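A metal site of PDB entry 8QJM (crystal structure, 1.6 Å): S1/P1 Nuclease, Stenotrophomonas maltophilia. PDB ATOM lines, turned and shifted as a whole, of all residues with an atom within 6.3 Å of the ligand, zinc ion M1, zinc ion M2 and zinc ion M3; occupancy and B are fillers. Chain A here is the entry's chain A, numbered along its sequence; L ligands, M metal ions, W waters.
Residues that only touch zinc ion M2: Arg 48. Within 4 Å of zinc ion M2: Asp 45, Arg 48, His 62, His 115 and Asp 119.
O1 of the ligand binds zinc ion M3 (1.9 Å). NE2 of His 125 is bound to zinc ion M3 (2.0 Å). Zinc ion M3 is bound by a ring nitrogen (NE2) of His 149. OD2 of Asp 153 binds zinc ion M3, 2.1 Å away. OD1 of Asp 153 binds zinc ion M3. Slightly farther from zinc ion M3 lies O3 of the ligand (2.8 Å).
The guanidinium group of Arg 48 is in hydrogen-bond range of an oxygen (O4) of the ligand, 3.0 Å away.
Four residues have an atom within 4 Å of zinc ion M3: Trp 1, His 125, His 149 and Asp 153. The nearest printed residue that does not touch zinc ion M3 is Gln 122 (4.4 Å).
ND1 of His 115 lies close to ND1 of His 6. A ring nitrogen (ND1) of His 125 sits at hydrogen-bond distance from the backbone carbonyl oxygen (O) of His 62 (2.7 Å). NH1 of Arg 48 sits close to ND1 of His 62, at 3.3 Å. N of His 149 sits at hydrogen-bond distance from OD1 of Asn 147 (3.1 Å). The backbone carbonyl oxygen (O) of Asp 153 is in hydrogen-bond range of the backbone NH (N) of Gly 2 (2.9 Å). N of Asp 153 sits close to NE2 of Gln 122 (3.2 Å). O of Gly 118 lies within hydrogen-bond range of NE1 of Trp 1, 2.8 Å away. OD1 of Asp 45 lies close to NH1 of Arg 48, 3.3 Å away.
Gly 2 touches the ligand. Ala 3 touches the ligand (N to O6, 3.7 Å). Gln 46 touches the ligand (NE2 to O7, 3.8 Å). Hydrophobic or aromatic side chains within 4 Å of the ligand: His 62 and His 125. 12 residues have an atom within 4 Å of the ligand: Trp 1, Gly 2, Ala 3, His 6, Asp 45, Gln 46, Arg 48, His 62, Asp 119, His 125, His 149 and Asp 153. Along chain A the residues within 4 Å of the ligand span positions 1 to 153. The nearest printed residue that does not touch the ligand is His 115 (4.03 Å).
Zinc ion M2 is bound by ND1 of His 62 (2.0 Å), NE2 of His 115 (2.0 Å), O2 of the ligand (2.0 Å), OD2 of Asp 119 (2.0 Å) and OD1 of Asp 45 (2.2 Å).
Water W1 lies within hydrogen-bond range of OD2 of Asp 45 (2.7 Å), O6 of the ligand (2.9 Å) and N of Ala 3 (3.4 Å). Water W5 lies within hydrogen-bond range of the side-chain hydroxyl (OG) of Ser 150 and the side-chain amide oxygen (OD1) of Asn 135.
Zinc ion M1 is bound by NE2 of His 6 (1.9 Å), O3 of the ligand (2.0 Å), OD1 of Asp 119 (2.1 Å), N of Trp 1 (2.2 Å) and O of Trp 1 (2.2 Å). Zinc ion M1 has five donor atoms within binding distance.
The nearest printed residue that does not touch zinc ion M1 is His 115 (4.1 Å).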
ATOM      1  N   TRP A   1      24.259 -16.543  -8.320  1.00  0.00           N
ATOM      2  CA  TRP A   1      23.255 -17.568  -7.836  1.00  0.00           C
ATOM      3  C   TRP A   1      23.987 -18.721  -7.155  1.00  0.00           C
ATOM      4  O   TRP A   1      25.162 -18.994  -7.512  1.00  0.00           O
ATOM      5  CB  TRP A   1      22.415 -18.112  -9.004  1.00  0.00           C
ATOM      6  CG  TRP A   1      21.733 -17.027  -9.776  1.00  0.00           C
ATOM      7  CD1 TRP A   1      22.082 -16.594 -11.024  1.00  0.00           C
ATOM      8  CD2 TRP A   1      20.616 -16.252  -9.361  1.00  0.00           C
ATOM      9  NE1 TRP A   1      21.252 -15.568 -11.381  1.00  0.00           N
ATOM     10  CE2 TRP A   1      20.361 -15.331 -10.381  1.00  0.00           C
ATOM     11  CE3 TRP A   1      19.811 -16.202  -8.221  1.00  0.00           C
ATOM     12  CZ2 TRP A   1      19.297 -14.432 -10.354  1.00  0.00           C
ATOM     13  CZ3 TRP A   1      18.794 -15.288  -8.152  1.00  0.00           C
ATOM     14  CH2 TRP A   1      18.532 -14.417  -9.216  1.00  0.00           C
ATOM     15  N   GLY A   2      23.254 -19.463  -6.315  1.00  0.00           N
ATOM     16  CA  GLY A   2      23.584 -20.815  -5.869  1.00  0.00           C
ATOM     17  C   GLY A   2      23.481 -21.772  -7.039  1.00  0.00           C
ATOM     18  O   GLY A   2      23.183 -21.357  -8.170  1.00  0.00           O
ATOM     19  N   ALA A   3      23.859 -23.006  -6.796  1.00  0.00           N
ATOM     20  CA  ALA A   3      23.979 -24.036  -7.829  1.00  0.00           C
ATOM     21  C   ALA A   3      22.631 -24.147  -8.543  1.00  0.00           C
ATOM     22  O   ALA A   3      22.643 -24.286  -9.780  1.00  0.00           O
ATOM     23  CB  ALA A   3      24.385 -25.377  -7.202  1.00  0.00           C
ATOM     24  N   HIS A   6      21.983 -21.394 -11.060  1.00  0.00           N
ATOM     25  CA  HIS A   6      22.834 -21.547 -12.276  1.00  0.00           C
ATOM     26  C   HIS A   6      22.191 -22.587 -13.185  1.00  0.00           C
ATOM     27  O   HIS A   6      22.184 -22.401 -14.445  1.00  0.00           O
ATOM     28  CB  HIS A   6      24.279 -21.835 -11.837  1.00  0.00           C
ATOM     29  CG  HIS A   6      24.944 -20.578 -11.413  1.00  0.00           C
ATOM     30  ND1 HIS A   6      25.263 -19.576 -12.313  1.00  0.00           N
ATOM     31  CD2 HIS A   6      25.295 -20.099 -10.185  1.00  0.00           C
ATOM     32  CE1 HIS A   6      25.776 -18.554 -11.647  1.00  0.00           C
ATOM     33  NE2 HIS A   6      25.806 -18.830 -10.380  1.00  0.00           N
ATOM     34  N   ALA A  44      32.042 -22.815 -12.537  1.00  0.00           N
ATOM     35  CA  ALA A  44      32.953 -21.676 -12.309  1.00  0.00           C
ATOM     36  C   ALA A  44      33.054 -21.380 -10.800  1.00  0.00           C
ATOM     37  O   ALA A  44      34.159 -21.000 -10.405  1.00  0.00           O
ATOM     38  CB  ALA A  44      32.525 -20.488 -13.139  1.00  0.00           C
ATOM     39  N   ASP A  45      32.018 -21.615  -9.992  1.00  0.00           N
ATOM     40  CA  ASP A  45      32.083 -21.394  -8.510  1.00  0.00           C
ATOM     41  C   ASP A  45      32.937 -22.487  -7.865  1.00  0.00           C
ATOM     42  O   ASP A  45      33.647 -22.172  -6.886  1.00  0.00           O
ATOM     43  CB  ASP A  45      30.700 -21.361  -7.863  1.00  0.00           C
ATOM     44  CG  ASP A  45      29.863 -20.184  -8.276  1.00  0.00           C
ATOM     45  OD1 ASP A  45      30.433 -19.149  -8.637  1.00  0.00           O
ATOM     46  OD2 ASP A  45      28.626 -20.291  -8.255  1.00  0.00           O
ATOM     47  N   GLN A  46      32.854 -23.711  -8.358  1.00  0.00           N
ATOM     48  CA  GLN A  46      33.655 -24.847  -7.853  1.00  0.00           C
ATOM     49  C   GLN A  46      35.130 -24.577  -8.202  1.00  0.00           C
ATOM     50  O   GLN A  46      35.967 -24.796  -7.345  1.00  0.00           O
ATOM     51  CB  GLN A  46      33.114 -26.169  -8.390  1.00  0.00           C
ATOM     52  CG  GLN A  46      31.821 -26.582  -7.717  1.00  0.00           C
ATOM     53  CD  GLN A  46      31.869 -26.325  -6.227  1.00  0.00           C
ATOM     54  OE1 GLN A  46      32.652 -26.947  -5.511  1.00  0.00           O
ATOM     55  NE2 GLN A  46      31.043 -25.424  -5.747  1.00  0.00           N
ATOM     56  N   ARG A  48      36.527 -21.657  -8.546  1.00  0.00           N
ATOM     57  CA  ARG A  48      36.941 -20.585  -7.576  1.00  0.00           C
ATOM     58  C   ARG A  48      37.270 -21.221  -6.213  1.00  0.00           C
ATOM     59  O   ARG A  48      38.316 -20.806  -5.579  1.00  0.00           O
ATOM     60  CB  ARG A  48      35.872 -19.474  -7.501  1.00  0.00           C
ATOM     61  CG  ARG A  48      36.247 -18.322  -6.575  1.00  0.00           C
ATOM     62  CD  ARG A  48      35.094 -17.359  -6.328  1.00  0.00           C
ATOM     63  NE  ARG A  48      34.006 -18.075  -5.723  1.00  0.00           N
ATOM     64  CZ  ARG A  48      32.721 -17.949  -6.046  1.00  0.00           C
ATOM     65  NH1 ARG A  48      32.319 -17.041  -6.931  1.00  0.00           N
ATOM     66  NH2 ARG A  48      31.829 -18.723  -5.453  1.00  0.00           N
ATOM     67  N   ALA A  49      36.462 -22.171  -5.755  1.00  0.00           N
ATOM     68  CA  ALA A  49      36.622 -22.827  -4.435  1.00  0.00           C
ATOM     69  C   ALA A  49      37.887 -23.680  -4.426  1.00  0.00           C
ATOM     70  O   ALA A  49      38.591 -23.669  -3.382  1.00  0.00           O
ATOM     71  CB  ALA A  49      35.424 -23.675  -4.084  1.00  0.00           C
ATOM     72  N   HIS A  62      33.074 -12.979 -11.364  1.00  0.00           N
ATOM     73  CA  HIS A  62      31.669 -13.339 -11.056  1.00  0.00           C
ATOM     74  C   HIS A  62      30.840 -12.087 -10.737  1.00  0.00           C
ATOM     75  O   HIS A  62      29.654 -12.241 -10.586  1.00  0.00           O
ATOM     76  CB  HIS A  62      31.569 -14.333  -9.895  1.00  0.00           C
ATOM     77  CG  HIS A  62      32.228 -15.635 -10.163  1.00  0.00           C
ATOM     78  ND1 HIS A  62      31.539 -16.844 -10.142  1.00  0.00           N
ATOM     79  CD2 HIS A  62      33.514 -15.919 -10.504  1.00  0.00           C
ATOM     80  CE1 HIS A  62      32.406 -17.805 -10.398  1.00  0.00           C
ATOM     81  NE2 HIS A  62      33.610 -17.276 -10.664  1.00  0.00           N
ATOM     82  N   HIS A 115      27.758 -19.817 -16.843  1.00  0.00           N
ATOM     83  CA  HIS A 115      27.831 -19.349 -15.441  1.00  0.00           C
ATOM     84  C   HIS A 115      27.616 -17.843 -15.392  1.00  0.00           C
ATOM     85  O   HIS A 115      26.854 -17.353 -14.480  1.00  0.00           O
ATOM     86  CB  HIS A 115      29.184 -19.731 -14.795  1.00  0.00           C
ATOM     87  CG  HIS A 115      29.141 -19.453 -13.314  1.00  0.00           C
ATOM     88  ND1 HIS A 115      28.600 -20.341 -12.384  1.00  0.00           N
ATOM     89  CD2 HIS A 115      29.502 -18.351 -12.635  1.00  0.00           C
ATOM     90  CE1 HIS A 115      28.684 -19.785 -11.167  1.00  0.00           C
ATOM     91  NE2 HIS A 115      29.211 -18.550 -11.309  1.00  0.00           N
ATOM     92  N   LEU A 116      28.353 -17.076 -16.206  1.00  0.00           N
ATOM     93  CA  LEU A 116      28.412 -15.617 -16.040  1.00  0.00           C
ATOM     94  C   LEU A 116      27.143 -14.940 -16.507  1.00  0.00           C
ATOM     95  O   LEU A 116      26.772 -13.929 -15.913  1.00  0.00           O
ATOM     96  CB  LEU A 116      29.646 -15.078 -16.749  1.00  0.00           C
ATOM     97  CG  LEU A 116      30.960 -15.538 -16.149  1.00  0.00           C
ATOM     98  CD1 LEU A 116      32.135 -14.999 -16.981  1.00  0.00           C
ATOM     99  CD2 LEU A 116      31.079 -15.155 -14.673  1.00  0.00           C
ATOM    100  N   GLY A 118      24.296 -16.252 -15.963  1.00  0.00           N
ATOM    101  CA  GLY A 118      23.609 -16.371 -14.659  1.00  0.00           C
ATOM    102  C   GLY A 118      23.986 -15.283 -13.655  1.00  0.00           C
ATOM    103  O   GLY A 118      23.115 -14.494 -13.167  1.00  0.00           O
ATOM    104  N   ASP A 119      25.259 -15.200 -13.272  1.00  0.00           N
ATOM    105  CA  ASP A 119      25.671 -14.280 -12.174  1.00  0.00           C
ATOM    106  C   ASP A 119      25.329 -12.819 -12.529  1.00  0.00           C
ATOM    107  O   ASP A 119      25.025 -12.053 -11.592  1.00  0.00           O
ATOM    108  CB  ASP A 119      27.160 -14.461 -11.875  1.00  0.00           C
ATOM    109  CG  ASP A 119      27.443 -15.560 -10.870  1.00  0.00           C
ATOM    110  OD1 ASP A 119      26.465 -16.019 -10.269  1.00  0.00           O
ATOM    111  OD2 ASP A 119      28.639 -15.890 -10.644  1.00  0.00           O
ATOM    112  N   GLN A 122      22.040 -11.654 -11.349  1.00  0.00           N
ATOM    113  CA  GLN A 122      21.795 -11.634  -9.871  1.00  0.00           C
ATOM    114  C   GLN A 122      22.090 -10.215  -9.421  1.00  0.00           C
ATOM    115  O   GLN A 122      23.241  -9.772  -9.486  1.00  0.00           O
ATOM    116  CB  GLN A 122      22.671 -12.704  -9.232  1.00  0.00           C
ATOM    117  CG  GLN A 122      22.103 -13.290  -7.924  1.00  0.00           C
ATOM    118  CD  GLN A 122      22.108 -12.328  -6.770  1.00  0.00           C
ATOM    119  OE1 GLN A 122      21.567 -11.225  -6.853  1.00  0.00           O
ATOM    120  NE2 GLN A 122      22.718 -12.742  -5.665  1.00  0.00           N
ATOM    121  N   HIS A 125      25.222  -9.145  -7.631  1.00  0.00           N
ATOM    122  CA  HIS A 125      26.514  -9.316  -8.341  1.00  0.00           C
ATOM    123  C   HIS A 125      26.853  -8.019  -9.093  1.00  0.00           C
ATOM    124  O   HIS A 125      27.889  -8.004  -9.766  1.00  0.00           O
ATOM    125  CB  HIS A 125      26.396 -10.518  -9.289  1.00  0.00           C
ATOM    126  CG  HIS A 125      26.581 -11.811  -8.574  1.00  0.00           C
ATOM    127  ND1 HIS A 125      27.671 -12.617  -8.859  1.00  0.00           N
ATOM    128  CD2 HIS A 125      25.907 -12.450  -7.581  1.00  0.00           C
ATOM    129  CE1 HIS A 125      27.663 -13.679  -8.080  1.00  0.00           C
ATOM    130  NE2 HIS A 125      26.571 -13.642  -7.333  1.00  0.00           N
ATOM    131  N   ASN A 135      27.601  -9.343   0.572  1.00  0.00           N
ATOM    132  CA  ASN A 135      28.208 -10.466   1.328  1.00  0.00           C
ATOM    133  C   ASN A 135      28.445  -9.992   2.766  1.00  0.00           C
ATOM    134  O   ASN A 135      28.260 -10.803   3.676  1.00  0.00           O
ATOM    135  CB  ASN A 135      29.471 -11.019   0.664  1.00  0.00           C
ATOM    136  CG  ASN A 135      29.160 -11.989  -0.454  1.00  0.00           C
ATOM    137  OD1 ASN A 135      28.649 -13.078  -0.208  1.00  0.00           O
ATOM    138  ND2 ASN A 135      29.471 -11.586  -1.683  1.00  0.00           N
ATOM    139  N   ASN A 147      23.270 -13.348   4.905  1.00  0.00           N
ATOM    140  CA  ASN A 147      23.705 -12.040   4.371  1.00  0.00           C
ATOM    141  C   ASN A 147      22.841 -11.779   3.148  1.00  0.00           C
ATOM    142  O   ASN A 147      22.273 -12.777   2.660  1.00  0.00           O
ATOM    143  CB  ASN A 147      25.209 -12.020   4.117  1.00  0.00           C
ATOM    144  CG  ASN A 147      25.640 -12.984   3.041  1.00  0.00           C
ATOM    145  OD1 ASN A 147      25.381 -12.754   1.875  1.00  0.00           O
ATOM    146  ND2 ASN A 147      26.313 -14.043   3.435  1.00  0.00           N
ATOM    147  N   HIS A 149      23.593 -10.974   0.091  1.00  0.00           N
ATOM    148  CA  HIS A 149      24.110 -11.720  -1.092  1.00  0.00           C
ATOM    149  C   HIS A 149      23.539 -13.151  -1.145  1.00  0.00           C
ATOM    150  O   HIS A 149      22.981 -13.538  -2.220  1.00  0.00           O
ATOM    151  CB  HIS A 149      25.652 -11.738  -1.084  1.00  0.00           C
ATOM    152  CG  HIS A 149      26.165 -12.166  -2.403  1.00  0.00           C
ATOM    153  ND1 HIS A 149      26.480 -11.260  -3.394  1.00  0.00           N
ATOM    154  CD2 HIS A 149      26.232 -13.406  -2.927  1.00  0.00           C
ATOM    155  CE1 HIS A 149      26.825 -11.944  -4.487  1.00  0.00           C
ATOM    156  NE2 HIS A 149      26.646 -13.300  -4.210  1.00  0.00           N
ATOM    157  N   SER A 150      23.711 -13.933  -0.078  1.00  0.00           N
ATOM    158  CA  SER A 150      23.261 -15.344   0.012  1.00  0.00           C
ATOM    159  C   SER A 150      21.737 -15.400  -0.144  1.00  0.00           C
ATOM    160  O   SER A 150      21.223 -16.372  -0.693  1.00  0.00           O
ATOM    161  CB  SER A 150      23.676 -15.961   1.341  1.00  0.00           C
ATOM    162  OG  SER A 150      25.103 -16.171   1.377  1.00  0.00           O
ATOM    163  N   ASP A 153      21.302 -15.024  -3.843  1.00  0.00           N
ATOM    164  CA  ASP A 153      21.892 -16.219  -4.530  1.00  0.00           C
ATOM    165  C   ASP A 153      20.968 -17.439  -4.351  1.00  0.00           C
ATOM    166  O   ASP A 153      20.802 -18.175  -5.353  1.00  0.00           O
ATOM    167  CB  ASP A 153      23.305 -16.532  -4.032  1.00  0.00           C
ATOM    168  CG  ASP A 153      24.453 -15.881  -4.782  1.00  0.00           C
ATOM    169  OD1 ASP A 153      24.221 -15.171  -5.761  1.00  0.00           O
ATOM    170  OD2 ASP A 153      25.574 -16.096  -4.364  1.00  0.00           O
HETATM  171  O1  LIG L   1      28.346 -15.525  -5.750  1.00  0.00           O
HETATM  172  P1  LIG L   1      28.477 -16.785  -6.790  1.00  0.00           P
HETATM  173  O2  LIG L   1      29.636 -16.607  -7.804  1.00  0.00           O
HETATM  174  O3  LIG L   1      27.096 -16.971  -7.288  1.00  0.00           O
HETATM  175  O4  LIG L   1      28.894 -18.111  -5.902  1.00  0.00           O
HETATM  176  C1  LIG L   1      27.844 -18.805  -5.223  1.00  0.00           C
HETATM  177  C2  LIG L   1      28.415 -20.089  -4.708  1.00  0.00           C
HETATM  178  O5  LIG L   1      29.473 -19.781  -3.769  1.00  0.00           O
HETATM  179  C3  LIG L   1      27.462 -20.977  -3.911  1.00  0.00           C
HETATM  180  O6  LIG L   1      26.770 -21.861  -4.789  1.00  0.00           O
HETATM  181  C4  LIG L   1      28.428 -21.792  -3.038  1.00  0.00           C
HETATM  182  O7  LIG L   1      29.057 -22.845  -3.746  1.00  0.00           O
HETATM  183  C5  LIG L   1      29.606 -20.833  -2.829  1.00  0.00           C
HETATM  184  N1  LIG L   1      29.639 -20.275  -1.462  1.00  0.00           N
HETATM  185  C6  LIG L   1      30.165 -21.082  -0.443  1.00  0.00           C
HETATM  186  N2  LIG L   1      30.170 -20.619   0.827  1.00  0.00           N
HETATM  187  C7  LIG L   1      29.685 -19.408   1.120  1.00  0.00           C
HETATM  188  C8  LIG L   1      29.133 -18.568   0.113  1.00  0.00           C
HETATM  189  C9  LIG L   1      29.129 -19.031  -1.158  1.00  0.00           C
HETATM  190  O8  LIG L   1      30.633 -22.190  -0.736  1.00  0.00           O
HETATM  191  N3  LIG L   1      29.712 -19.012   2.395  1.00  0.00           N
HETATM  192 ZN    ZN M   1      26.069 -17.591  -8.898  1.00  0.00          ZN
HETATM  193 ZN    ZN M   2      29.647 -17.398  -9.691  1.00  0.00          ZN
HETATM  194 ZN    ZN M   3      26.617 -14.745  -5.653  1.00  0.00          ZN
HETATM  195  O   HOH W   1      27.122 -22.413  -7.606  1.00  0.00           O
HETATM  196  O   HOH W   2      27.393 -24.892  -4.374  1.00  0.00           O
HETATM  197  O   HOH W   3      30.707 -13.508  -6.351  1.00  0.00           O
HETATM  198  O   HOH W   4      26.052 -17.679  -2.124  1.00  0.00           O
HETATM  199  O   HOH W   5      27.078 -16.160  -0.389  1.00  0.00           O
